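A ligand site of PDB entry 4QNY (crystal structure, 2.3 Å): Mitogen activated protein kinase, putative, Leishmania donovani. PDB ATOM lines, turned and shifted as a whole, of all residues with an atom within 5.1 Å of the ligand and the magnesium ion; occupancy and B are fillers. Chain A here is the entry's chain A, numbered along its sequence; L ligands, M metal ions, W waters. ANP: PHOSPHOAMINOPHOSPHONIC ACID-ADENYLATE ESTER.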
ATOM      1  N   ILE A  28       2.595  -6.080  14.750  1.00  0.00           N
ATOM      2  CA  ILE A  28       2.281  -5.254  15.916  1.00  0.00           C
ATOM      3  C   ILE A  28       1.907  -6.079  17.139  1.00  0.00           C
ATOM      4  O   ILE A  28       1.863  -5.559  18.256  1.00  0.00           O
ATOM      5  CB  ILE A  28       1.126  -4.286  15.611  1.00  0.00           C
ATOM      6  CG1 ILE A  28      -0.037  -5.039  14.958  1.00  0.00           C
ATOM      7  CG2 ILE A  28       1.598  -3.169  14.693  1.00  0.00           C
ATOM      8  CD1 ILE A  28      -1.280  -4.205  14.759  1.00  0.00           C
ATOM      9  N   GLY A  29       1.633  -7.362  16.933  1.00  0.00           N
ATOM     10  CA  GLY A  29       1.224  -8.233  18.022  1.00  0.00           C
ATOM     11  C   GLY A  29       1.672  -9.659  17.846  1.00  0.00           C
ATOM     12  O   GLY A  29       1.707 -10.183  16.726  1.00  0.00           O
ATOM     13  N   ALA A  30       2.024 -10.313  18.954  1.00  0.00           N
ATOM     14  CA  ALA A  30       2.426 -11.710  18.935  1.00  0.00           C
ATOM     15  C   ALA A  30       1.608 -12.514  19.942  1.00  0.00           C
ATOM     16  O   ALA A  30       1.493 -12.145  21.109  1.00  0.00           O
ATOM     17  CB  ALA A  30       3.908 -11.834  19.238  1.00  0.00           C
ATOM     18  N   GLY A  31       1.023 -13.612  19.474  1.00  0.00           N
ATOM     19  CA  GLY A  31       0.219 -14.469  20.317  1.00  0.00           C
ATOM     20  C   GLY A  31       0.767 -15.879  20.408  1.00  0.00           C
ATOM     21  O   GLY A  31       1.771 -16.197  19.778  1.00  0.00           O
ATOM     22  N   SER A  32       0.092 -16.718  21.192  1.00  0.00           N
ATOM     23  CA  SER A  32       0.520 -18.099  21.362  1.00  0.00           C
ATOM     24  C   SER A  32       0.186 -18.940  20.141  1.00  0.00           C
ATOM     25  O   SER A  32       0.840 -19.955  19.876  1.00  0.00           O
ATOM     26  CB  SER A  32      -0.140 -18.702  22.614  1.00  0.00           C
ATOM     27  OG  SER A  32       0.161 -17.940  23.766  1.00  0.00           O
ATOM     28  N   GLY A  34      -0.554 -17.349  16.870  1.00  0.00           N
ATOM     29  CA  GLY A  34      -0.556 -16.486  15.693  1.00  0.00           C
ATOM     30  C   GLY A  34      -0.115 -15.063  15.942  1.00  0.00           C
ATOM     31  O   GLY A  34      -0.178 -14.564  17.070  1.00  0.00           O
ATOM     32  N   VAL A  36      -0.084 -10.768  14.926  1.00  0.00           N
ATOM     33  CA  VAL A  36      -0.963  -9.683  14.514  1.00  0.00           C
ATOM     34  C   VAL A  36      -0.171  -8.672  13.683  1.00  0.00           C
ATOM     35  O   VAL A  36       0.884  -8.196  14.104  1.00  0.00           O
ATOM     36  CB  VAL A  36      -1.602  -8.963  15.719  1.00  0.00           C
ATOM     37  CG1 VAL A  36      -2.502  -7.832  15.251  1.00  0.00           C
ATOM     38  CG2 VAL A  36      -2.383  -9.955  16.560  1.00  0.00           C
ATOM     39  N   ALA A  50      -5.754  -4.011  10.839  1.00  0.00           N
ATOM     40  CA  ALA A  50      -5.073  -5.057  11.589  1.00  0.00           C
ATOM     41  C   ALA A  50      -5.423  -6.451  11.060  1.00  0.00           C
ATOM     42  O   ALA A  50      -6.580  -6.738  10.770  1.00  0.00           O
ATOM     43  CB  ALA A  50      -5.400  -4.953  13.072  1.00  0.00           C
ATOM     44  N   LYS A  52      -4.993 -10.571  11.900  1.00  0.00           N
ATOM     45  CA  LYS A  52      -4.654 -11.572  12.907  1.00  0.00           C
ATOM     46  C   LYS A  52      -4.560 -12.966  12.291  1.00  0.00           C
ATOM     47  O   LYS A  52      -5.563 -13.551  11.885  1.00  0.00           O
ATOM     48  CB  LYS A  52      -5.709 -11.559  14.017  1.00  0.00           C
ATOM     49  CG  LYS A  52      -5.416 -12.482  15.185  1.00  0.00           C
ATOM     50  CD  LYS A  52      -6.483 -12.336  16.268  1.00  0.00           C
ATOM     51  CE  LYS A  52      -6.191 -13.204  17.472  1.00  0.00           C
ATOM     52  NZ  LYS A  52      -7.202 -13.017  18.544  1.00  0.00           N
ATOM     53  N   ILE A  68     -11.745 -20.469  18.221  1.00  0.00           N
ATOM     54  CA  ILE A  68     -11.470 -19.439  17.221  1.00  0.00           C
ATOM     55  C   ILE A  68     -12.722 -19.174  16.385  1.00  0.00           C
ATOM     56  O   ILE A  68     -12.971 -18.045  15.982  1.00  0.00           O
ATOM     57  CB  ILE A  68     -10.268 -19.820  16.312  1.00  0.00           C
ATOM     58  CG1 ILE A  68      -9.686 -18.563  15.651  1.00  0.00           C
ATOM     59  CG2 ILE A  68     -10.643 -20.869  15.280  1.00  0.00           C
ATOM     60  CD1 ILE A  68      -9.013 -17.619  16.612  1.00  0.00           C
ATOM     61  N   GLU A  71     -14.907 -16.919  18.325  1.00  0.00           N
ATOM     62  CA  GLU A  71     -14.321 -15.586  18.376  1.00  0.00           C
ATOM     63  C   GLU A  71     -14.685 -14.762  17.140  1.00  0.00           C
ATOM     64  O   GLU A  71     -15.027 -13.590  17.252  1.00  0.00           O
ATOM     65  CB  GLU A  71     -12.799 -15.669  18.526  1.00  0.00           C
ATOM     66  CG  GLU A  71     -12.109 -14.317  18.613  1.00  0.00           C
ATOM     67  CD  GLU A  71     -10.605 -14.432  18.755  1.00  0.00           C
ATOM     68  OE1 GLU A  71     -10.115 -15.544  19.075  1.00  0.00           O
ATOM     69  OE2 GLU A  71      -9.908 -13.421  18.554  1.00  0.00           O
ATOM     70  N   ILE A  84     -13.863  -3.944  19.230  1.00  0.00           N
ATOM     71  CA  ILE A  84     -13.087  -3.977  18.000  1.00  0.00           C
ATOM     72  C   ILE A  84     -13.892  -4.647  16.873  1.00  0.00           C
ATOM     73  O   ILE A  84     -14.491  -5.707  17.050  1.00  0.00           O
ATOM     74  CB  ILE A  84     -11.723  -4.692  18.200  1.00  0.00           C
ATOM     75  CG1 ILE A  84     -10.824  -4.474  16.978  1.00  0.00           C
ATOM     76  CG2 ILE A  84     -11.901  -6.172  18.509  1.00  0.00           C
ATOM     77  CD1 ILE A  84     -10.344  -3.040  16.830  1.00  0.00           C
ATOM     78  N   MET A 105      -9.270  -6.948  11.169  1.00  0.00           N
ATOM     79  CA  MET A 105      -9.981  -6.054  12.063  1.00  0.00           C
ATOM     80  C   MET A 105      -9.558  -4.601  11.864  1.00  0.00           C
ATOM     81  O   MET A 105      -8.550  -4.327  11.213  1.00  0.00           O
ATOM     82  CB  MET A 105      -9.736  -6.450  13.514  1.00  0.00           C
ATOM     83  CG  MET A 105      -9.937  -7.924  13.819  1.00  0.00           C
ATOM     84  SD  MET A 105      -9.069  -8.430  15.316  1.00  0.00           S
ATOM     85  CE  MET A 105      -7.369  -8.170  14.818  1.00  0.00           C
ATOM     86  N   ASP A 106     -10.341  -3.682  12.429  1.00  0.00           N
ATOM     87  CA  ASP A 106      -9.951  -2.272  12.462  1.00  0.00           C
ATOM     88  C   ASP A 106      -8.664  -2.112  13.255  1.00  0.00           C
ATOM     89  O   ASP A 106      -8.375  -2.894  14.152  1.00  0.00           O
ATOM     90  CB  ASP A 106     -11.057  -1.409  13.069  1.00  0.00           C
ATOM     91  CG  ASP A 106     -12.287  -1.326  12.190  1.00  0.00           C
ATOM     92  OD1 ASP A 106     -12.123  -1.151  10.961  1.00  0.00           O
ATOM     93  OD2 ASP A 106     -13.411  -1.427  12.715  1.00  0.00           O
ATOM     94  N   ILE A 107      -7.885  -1.081  12.932  1.00  0.00           N
ATOM     95  CA  ILE A 107      -6.599  -0.872  13.582  1.00  0.00           C
ATOM     96  C   ILE A 107      -6.724   0.101  14.752  1.00  0.00           C
ATOM     97  O   ILE A 107      -7.444   1.104  14.682  1.00  0.00           O
ATOM     98  CB  ILE A 107      -5.537  -0.361  12.579  1.00  0.00           C
ATOM     99  CG1 ILE A 107      -4.151  -0.314  13.232  1.00  0.00           C
ATOM    100  CG2 ILE A 107      -5.923   0.988  11.994  1.00  0.00           C
ATOM    101  CD1 ILE A 107      -3.624  -1.657  13.647  1.00  0.00           C
ATOM    102  N   MET A 108      -6.039  -0.212  15.847  1.00  0.00           N
ATOM    103  CA  MET A 108      -5.926   0.688  16.983  1.00  0.00           C
ATOM    104  C   MET A 108      -4.446   0.983  17.227  1.00  0.00           C
ATOM    105  O   MET A 108      -3.585   0.183  16.872  1.00  0.00           O
ATOM    106  CB  MET A 108      -6.589   0.102  18.225  1.00  0.00           C
ATOM    107  CG  MET A 108      -8.093  -0.075  18.100  1.00  0.00           C
ATOM    108  SD  MET A 108      -8.991   1.491  18.068  1.00  0.00           S
ATOM    109  CE  MET A 108      -8.799   2.022  19.772  1.00  0.00           C
ATOM    110  N   ASP A 111      -2.291  -0.781  23.052  1.00  0.00           N
ATOM    111  CA  ASP A 111      -3.185  -1.275  24.105  1.00  0.00           C
ATOM    112  C   ASP A 111      -2.682  -0.853  25.490  1.00  0.00           C
ATOM    113  O   ASP A 111      -1.601  -0.264  25.620  1.00  0.00           O
ATOM    114  CB  ASP A 111      -3.351  -2.793  24.022  1.00  0.00           C
ATOM    115  CG  ASP A 111      -2.058  -3.550  24.214  1.00  0.00           C
ATOM    116  OD1 ASP A 111      -1.392  -3.345  25.246  1.00  0.00           O
ATOM    117  OD2 ASP A 111      -1.696  -4.360  23.335  1.00  0.00           O
ATOM    118  N   GLN A 114       1.168  -2.305  27.306  1.00  0.00           N
ATOM    119  CA  GLN A 114       1.932  -1.162  26.684  1.00  0.00           C
ATOM    120  C   GLN A 114       1.935   0.218  27.237  1.00  0.00           C
ATOM    121  O   GLN A 114       2.996   0.794  27.435  1.00  0.00           O
ATOM    122  CB  GLN A 114       1.484  -0.970  25.235  1.00  0.00           C
ATOM    123  CG  GLN A 114       2.399  -1.448  23.943  1.00  0.00           C
ATOM    124  CD  GLN A 114       1.744  -2.649  23.250  1.00  0.00           C
ATOM    125  OE1 GLN A 114       0.568  -2.765  23.533  1.00  0.00           O
ATOM    126  NE2 GLN A 114       2.368  -3.283  22.207  1.00  0.00           N
ATOM    127  N   ASP A 150     -11.589 -12.955  29.583  1.00  0.00           N
ATOM    128  CA  ASP A 150     -10.177 -12.605  29.424  1.00  0.00           C
ATOM    129  C   ASP A 150      -9.944 -11.095  29.425  1.00  0.00           C
ATOM    130  O   ASP A 150      -9.270 -10.571  28.532  1.00  0.00           O
ATOM    131  CB  ASP A 150      -9.629 -13.226  28.139  1.00  0.00           C
ATOM    132  CG  ASP A 150      -8.120 -13.398  28.174  1.00  0.00           C
ATOM    133  OD1 ASP A 150      -7.550 -13.447  29.286  1.00  0.00           O
ATOM    134  OD2 ASP A 150      -7.504 -13.485  27.098  1.00  0.00           O
ATOM    135  N   ALA A 154      -3.777  -6.076  28.041  1.00  0.00           N
ATOM    136  CA  ALA A 154      -3.331  -6.418  26.690  1.00  0.00           C
ATOM    137  C   ALA A 154      -4.510  -6.593  25.743  1.00  0.00           C
ATOM    138  O   ALA A 154      -4.370  -6.427  24.530  1.00  0.00           O
ATOM    139  CB  ALA A 154      -2.480  -7.680  26.725  1.00  0.00           C
ATOM    140  N   ASN A 155      -5.667  -6.942  26.296  1.00  0.00           N
ATOM    141  CA  ASN A 155      -6.872  -7.132  25.500  1.00  0.00           C
ATOM    142  C   ASN A 155      -7.747  -5.876  25.443  1.00  0.00           C
ATOM    143  O   ASN A 155      -8.909  -5.935  25.064  1.00  0.00           O
ATOM    144  CB  ASN A 155      -7.692  -8.311  26.034  1.00  0.00           C
ATOM    145  CG  ASN A 155      -6.968  -9.639  25.869  1.00  0.00           C
ATOM    146  OD1 ASN A 155      -6.039  -9.756  25.063  1.00  0.00           O
ATOM    147  ND2 ASN A 155      -7.381 -10.646  26.625  1.00  0.00           N
ATOM    148  N   LEU A 157      -7.700  -2.210  23.694  1.00  0.00           N
ATOM    149  CA  LEU A 157      -7.041  -1.381  22.686  1.00  0.00           C
ATOM    150  C   LEU A 157      -7.421   0.098  22.804  1.00  0.00           C
ATOM    151  O   LEU A 157      -8.592   0.440  22.991  1.00  0.00           O
ATOM    152  CB  LEU A 157      -7.382  -1.880  21.289  1.00  0.00           C
ATOM    153  CG  LEU A 157      -6.977  -3.332  20.978  1.00  0.00           C
ATOM    154  CD1 LEU A 157      -7.532  -3.763  19.618  1.00  0.00           C
ATOM    155  CD2 LEU A 157      -5.465  -3.488  21.020  1.00  0.00           C
ATOM    156  N   CYS A 167     -10.888  -6.275  22.787  1.00  0.00           N
ATOM    157  CA  CYS A 167     -10.596  -7.320  21.801  1.00  0.00           C
ATOM    158  C   CYS A 167     -10.382  -8.683  22.468  1.00  0.00           C
ATOM    159  O   CYS A 167     -10.571  -8.831  23.671  1.00  0.00           O
ATOM    160  CB  CYS A 167      -9.350  -6.948  20.982  1.00  0.00           C
ATOM    161  SG  CYS A 167      -7.799  -6.994  21.911  1.00  0.00           S
ATOM    162  N   ASP A 168     -10.014  -9.669  21.645  1.00  0.00           N
ATOM    163  CA  ASP A 168      -9.688 -11.026  22.091  1.00  0.00           C
ATOM    164  C   ASP A 168     -10.862 -11.735  22.753  1.00  0.00           C
ATOM    165  O   ASP A 168     -10.939 -11.838  23.973  1.00  0.00           O
ATOM    166  CB  ASP A 168      -8.489 -10.991  23.048  1.00  0.00           C
ATOM    167  CG  ASP A 168      -7.823 -12.348  23.193  1.00  0.00           C
ATOM    168  OD1 ASP A 168      -8.456 -13.370  22.860  1.00  0.00           O
ATOM    169  OD2 ASP A 168      -6.657 -12.390  23.641  1.00  0.00           O
ATOM    170  N   GLY A 170     -11.313 -14.859  22.511  1.00  0.00           N
ATOM    171  CA  GLY A 170     -10.846 -16.230  22.346  1.00  0.00           C
ATOM    172  C   GLY A 170     -11.221 -17.170  23.484  1.00  0.00           C
ATOM    173  O   GLY A 170     -11.184 -18.387  23.321  1.00  0.00           O
HETATM  174  PG  ANP L   1      -6.145 -15.371  20.977  1.00  0.00           P
HETATM  175  O1G ANP L   1      -5.332 -15.419  19.725  1.00  0.00           O
HETATM  176  O2G ANP L   1      -7.645 -15.065  20.610  1.00  0.00           O
HETATM  177  O3G ANP L   1      -6.079 -16.784  21.695  1.00  0.00           O
HETATM  178  PB  ANP L   1      -4.284 -13.288  21.439  1.00  0.00           P
HETATM  179  O1B ANP L   1      -3.229 -14.196  20.897  1.00  0.00           O
HETATM  180  O2B ANP L   1      -3.663 -12.453  22.601  1.00  0.00           O
HETATM  181  N3B ANP L   1      -5.578 -14.182  22.043  1.00  0.00           N
HETATM  182  PA  ANP L   1      -5.160 -10.817  20.554  1.00  0.00           P
HETATM  183  O1A ANP L   1      -5.262 -10.503  21.995  1.00  0.00           O
HETATM  184  O2A ANP L   1      -6.463 -10.573  19.785  1.00  0.00           O
HETATM  185  O3A ANP L   1      -4.778 -12.346  20.300  1.00  0.00           O
HETATM  186  O5' ANP L   1      -3.980  -9.948  19.948  1.00  0.00           O
HETATM  187  C5' ANP L   1      -2.679  -9.898  20.577  1.00  0.00           C
HETATM  188  C4' ANP L   1      -2.191  -8.467  20.568  1.00  0.00           C
HETATM  189  O4' ANP L   1      -2.285  -7.913  19.243  1.00  0.00           O
HETATM  190  C3' ANP L   1      -2.988  -7.510  21.439  1.00  0.00           C
HETATM  191  O3' ANP L   1      -2.553  -7.559  22.794  1.00  0.00           O
HETATM  192  C2' ANP L   1      -2.680  -6.154  20.791  1.00  0.00           C
HETATM  193  O2' ANP L   1      -1.451  -5.606  21.277  1.00  0.00           O
HETATM  194  C1' ANP L   1      -2.548  -6.531  19.308  1.00  0.00           C
HETATM  195  N9  ANP L   1      -3.758  -6.251  18.526  1.00  0.00           N
HETATM  196  C8  ANP L   1      -4.830  -7.070  18.353  1.00  0.00           C
HETATM  197  N7  ANP L   1      -5.779  -6.567  17.605  1.00  0.00           N
HETATM  198  C5  ANP L   1      -5.293  -5.314  17.270  1.00  0.00           C
HETATM  199  C6  ANP L   1      -5.826  -4.265  16.490  1.00  0.00           C
HETATM  200  N6  ANP L   1      -7.011  -4.321  15.891  1.00  0.00           N
HETATM  201  N1  ANP L   1      -5.087  -3.147  16.364  1.00  0.00           N
HETATM  202  C2  ANP L   1      -3.896  -3.078  16.962  1.00  0.00           C
HETATM  203  N3  ANP L   1      -3.293  -4.005  17.727  1.00  0.00           N
HETATM  204  C4  ANP L   1      -4.046  -5.101  17.836  1.00  0.00           C
HETATM  205 MG    MG M   1      -4.976 -11.074  23.872  1.00  0.00          MG
HETATM  206  O   HOH W   1      -8.796  -9.376  18.699  1.00  0.00           O
HETATM  207  O   HOH W   2      -4.663 -16.038  16.933  1.00  0.00           O
HETATM  208  O   HOH W   3      -3.292  -9.928  24.068  1.00  0.00           O
HETATM  209  O   HOH W   4      -3.227 -16.783  21.804  1.00  0.00           O
HETATM  210  O   HOH W   5      -0.247  -2.663  20.704  1.00  0.00           O
HETATM  211  O   HOH W   6      -2.464 -15.066  18.436  1.00  0.00           O
HETATM  212  O   HOH W   7      -4.526 -12.007  25.556  1.00  0.00           O
HETATM  213  O   HOH W   8      -0.925 -12.996  24.369  1.00  0.00           O
HETATM  214  O   HOH W   9       1.530  -6.534  21.333  1.00  0.00           O
HETATM  215  O   HOH W  10      -7.499 -16.063  24.178  1.00  0.00           O
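The backbone NH (N) of Cys 167 lies within hydrogen-bond range of the backbone carbonyl oxygen (O) of Asn 155 (3.0 Å).
The backbone carbonyl oxygen (O) of Asp 150 lies within hydrogen-bond range of the side-chain amide nitrogen (ND2) of Asn 155, at 2.7 Å.
N of Gly 170 lies close to OD1 of Asp 168, 3.2 Å away.
OD1 of Asp 111 sits close to OE1 of Gln 114 (2.7 Å).
The side-chain carboxylate (OE2) of Glu 71 lies within salt-bridge range of the side-chain amino group (NZ) of Lys 52.
The backbone carbonyl oxygen (O) of Ala 50 lies within hydrogen-bond range of the backbone NH (N) of Met 105.
O of Val 36 lies within hydrogen-bond range of N of Ile 28, at 2.8 Å.
N of Val 36 sits at hydrogen-bond distance from O of Gly 29 (2.6 Å).
CD1 of Ile 28 touches N3 of the ligand, 3.6 Å away.
Gly 29 touches the ligand.
CA of Gly 31 touches O1B of the ligand, 3.5 Å away.
CG2 of Val 36 touches O4' of the ligand, 3.4 Å away.
CB of Ala 50 touches N6 of the ligand (3.3 Å).
CD1 of Ile 84 touches N6 of the ligand, at 3.7 Å.
CE of Met 105 touches N7 of the ligand, at 3.6 Å.
Ile 107 touches the ligand.
Leu 157 touches the ligand (CD1 to C5, 3.6 Å).
Gly 170 touches the ligand (CA to O2G, 3.8 Å).
Within 4 Å of the ligand: Ile 28, Gly 29, Gly 31, Val 36, Ala 50, Lys 52, Glu 71, Ile 84, Met 105, Asp 106, Ile 107, Met 108, Asp 111, Ala 154, Asn 155, Leu 157, Asp 168 and Gly 170.
The magnesium ion is bound by water W7 (2.0 Å), O1A of the ligand (2.0 Å), water W3 (2.0 Å), OD1 of Asn 155 (2.1 Å), OD2 of Asp 168 (2.1 Å) and O2B of the ligand (2.3 Å).
The magnesium ion has six donor atoms within binding distance.
The side-chain carboxylate of Asp 111 sits at hydrogen-bond distance from an oxygen (O2') of the ligand (2.4 Å).
The backbone carbonyl oxygen of Asp 106 sits at hydrogen-bond distance from a nitrogen (N6) of the ligand (2.6 Å).
An oxygen (O3') of the ligand sits at hydrogen-bond distance from the backbone carbonyl oxygen (O) of Ala 154 (2.8 Å).
An oxygen (O2A) of the ligand is in salt-bridge range of the side-chain amino group of Lys 52, 2.8 Å away.
The side-chain carboxylate of Glu 71 lies close to an oxygen (O2G) of the ligand, 2.9 Å away.
The backbone NH (N) of Met 108 sits at hydrogen-bond distance from a nitrogen (N1) of the ligand (3.1 Å).
Water W6 bridges O of Gly 34 (2.7 Å) and O1B of the ligand (2.7 Å).
Water W4 bridges O1B of the ligand (2.7 Å) and N of Ser 32 (3.4 Å).
Water W1 lies within hydrogen-bond range of an oxygen (O2A) of the ligand (2.8 Å), the backbone NH (N) of Asp 168 (3.2 Å) and the side-chain sulfur (SD) of Met 105 (3.5 Å).
Water W10 bridges O3G of the ligand (2.9 Å) and OD1 of Asp 168 (3.1 Å).
Water W9 lies within hydrogen-bond range of O2' of the ligand (3.1 Å), O of Ile 28 (3.2 Å) and NE2 of Gln 114 (3.5 Å).
Water W5 lies within hydrogen-bond range of the side-chain amide oxygen of Gln 114 (2.9 Å), an oxygen (O2') of the ligand (3.2 Å) and the side-chain carboxylate of Asp 111 (3.4 Å).
Of the 25 residues printed, 2 come within 4 Å of the magnesium ion.
The nearest printed residue that does not touch the magnesium ion is Ala 154 (4.7 Å).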
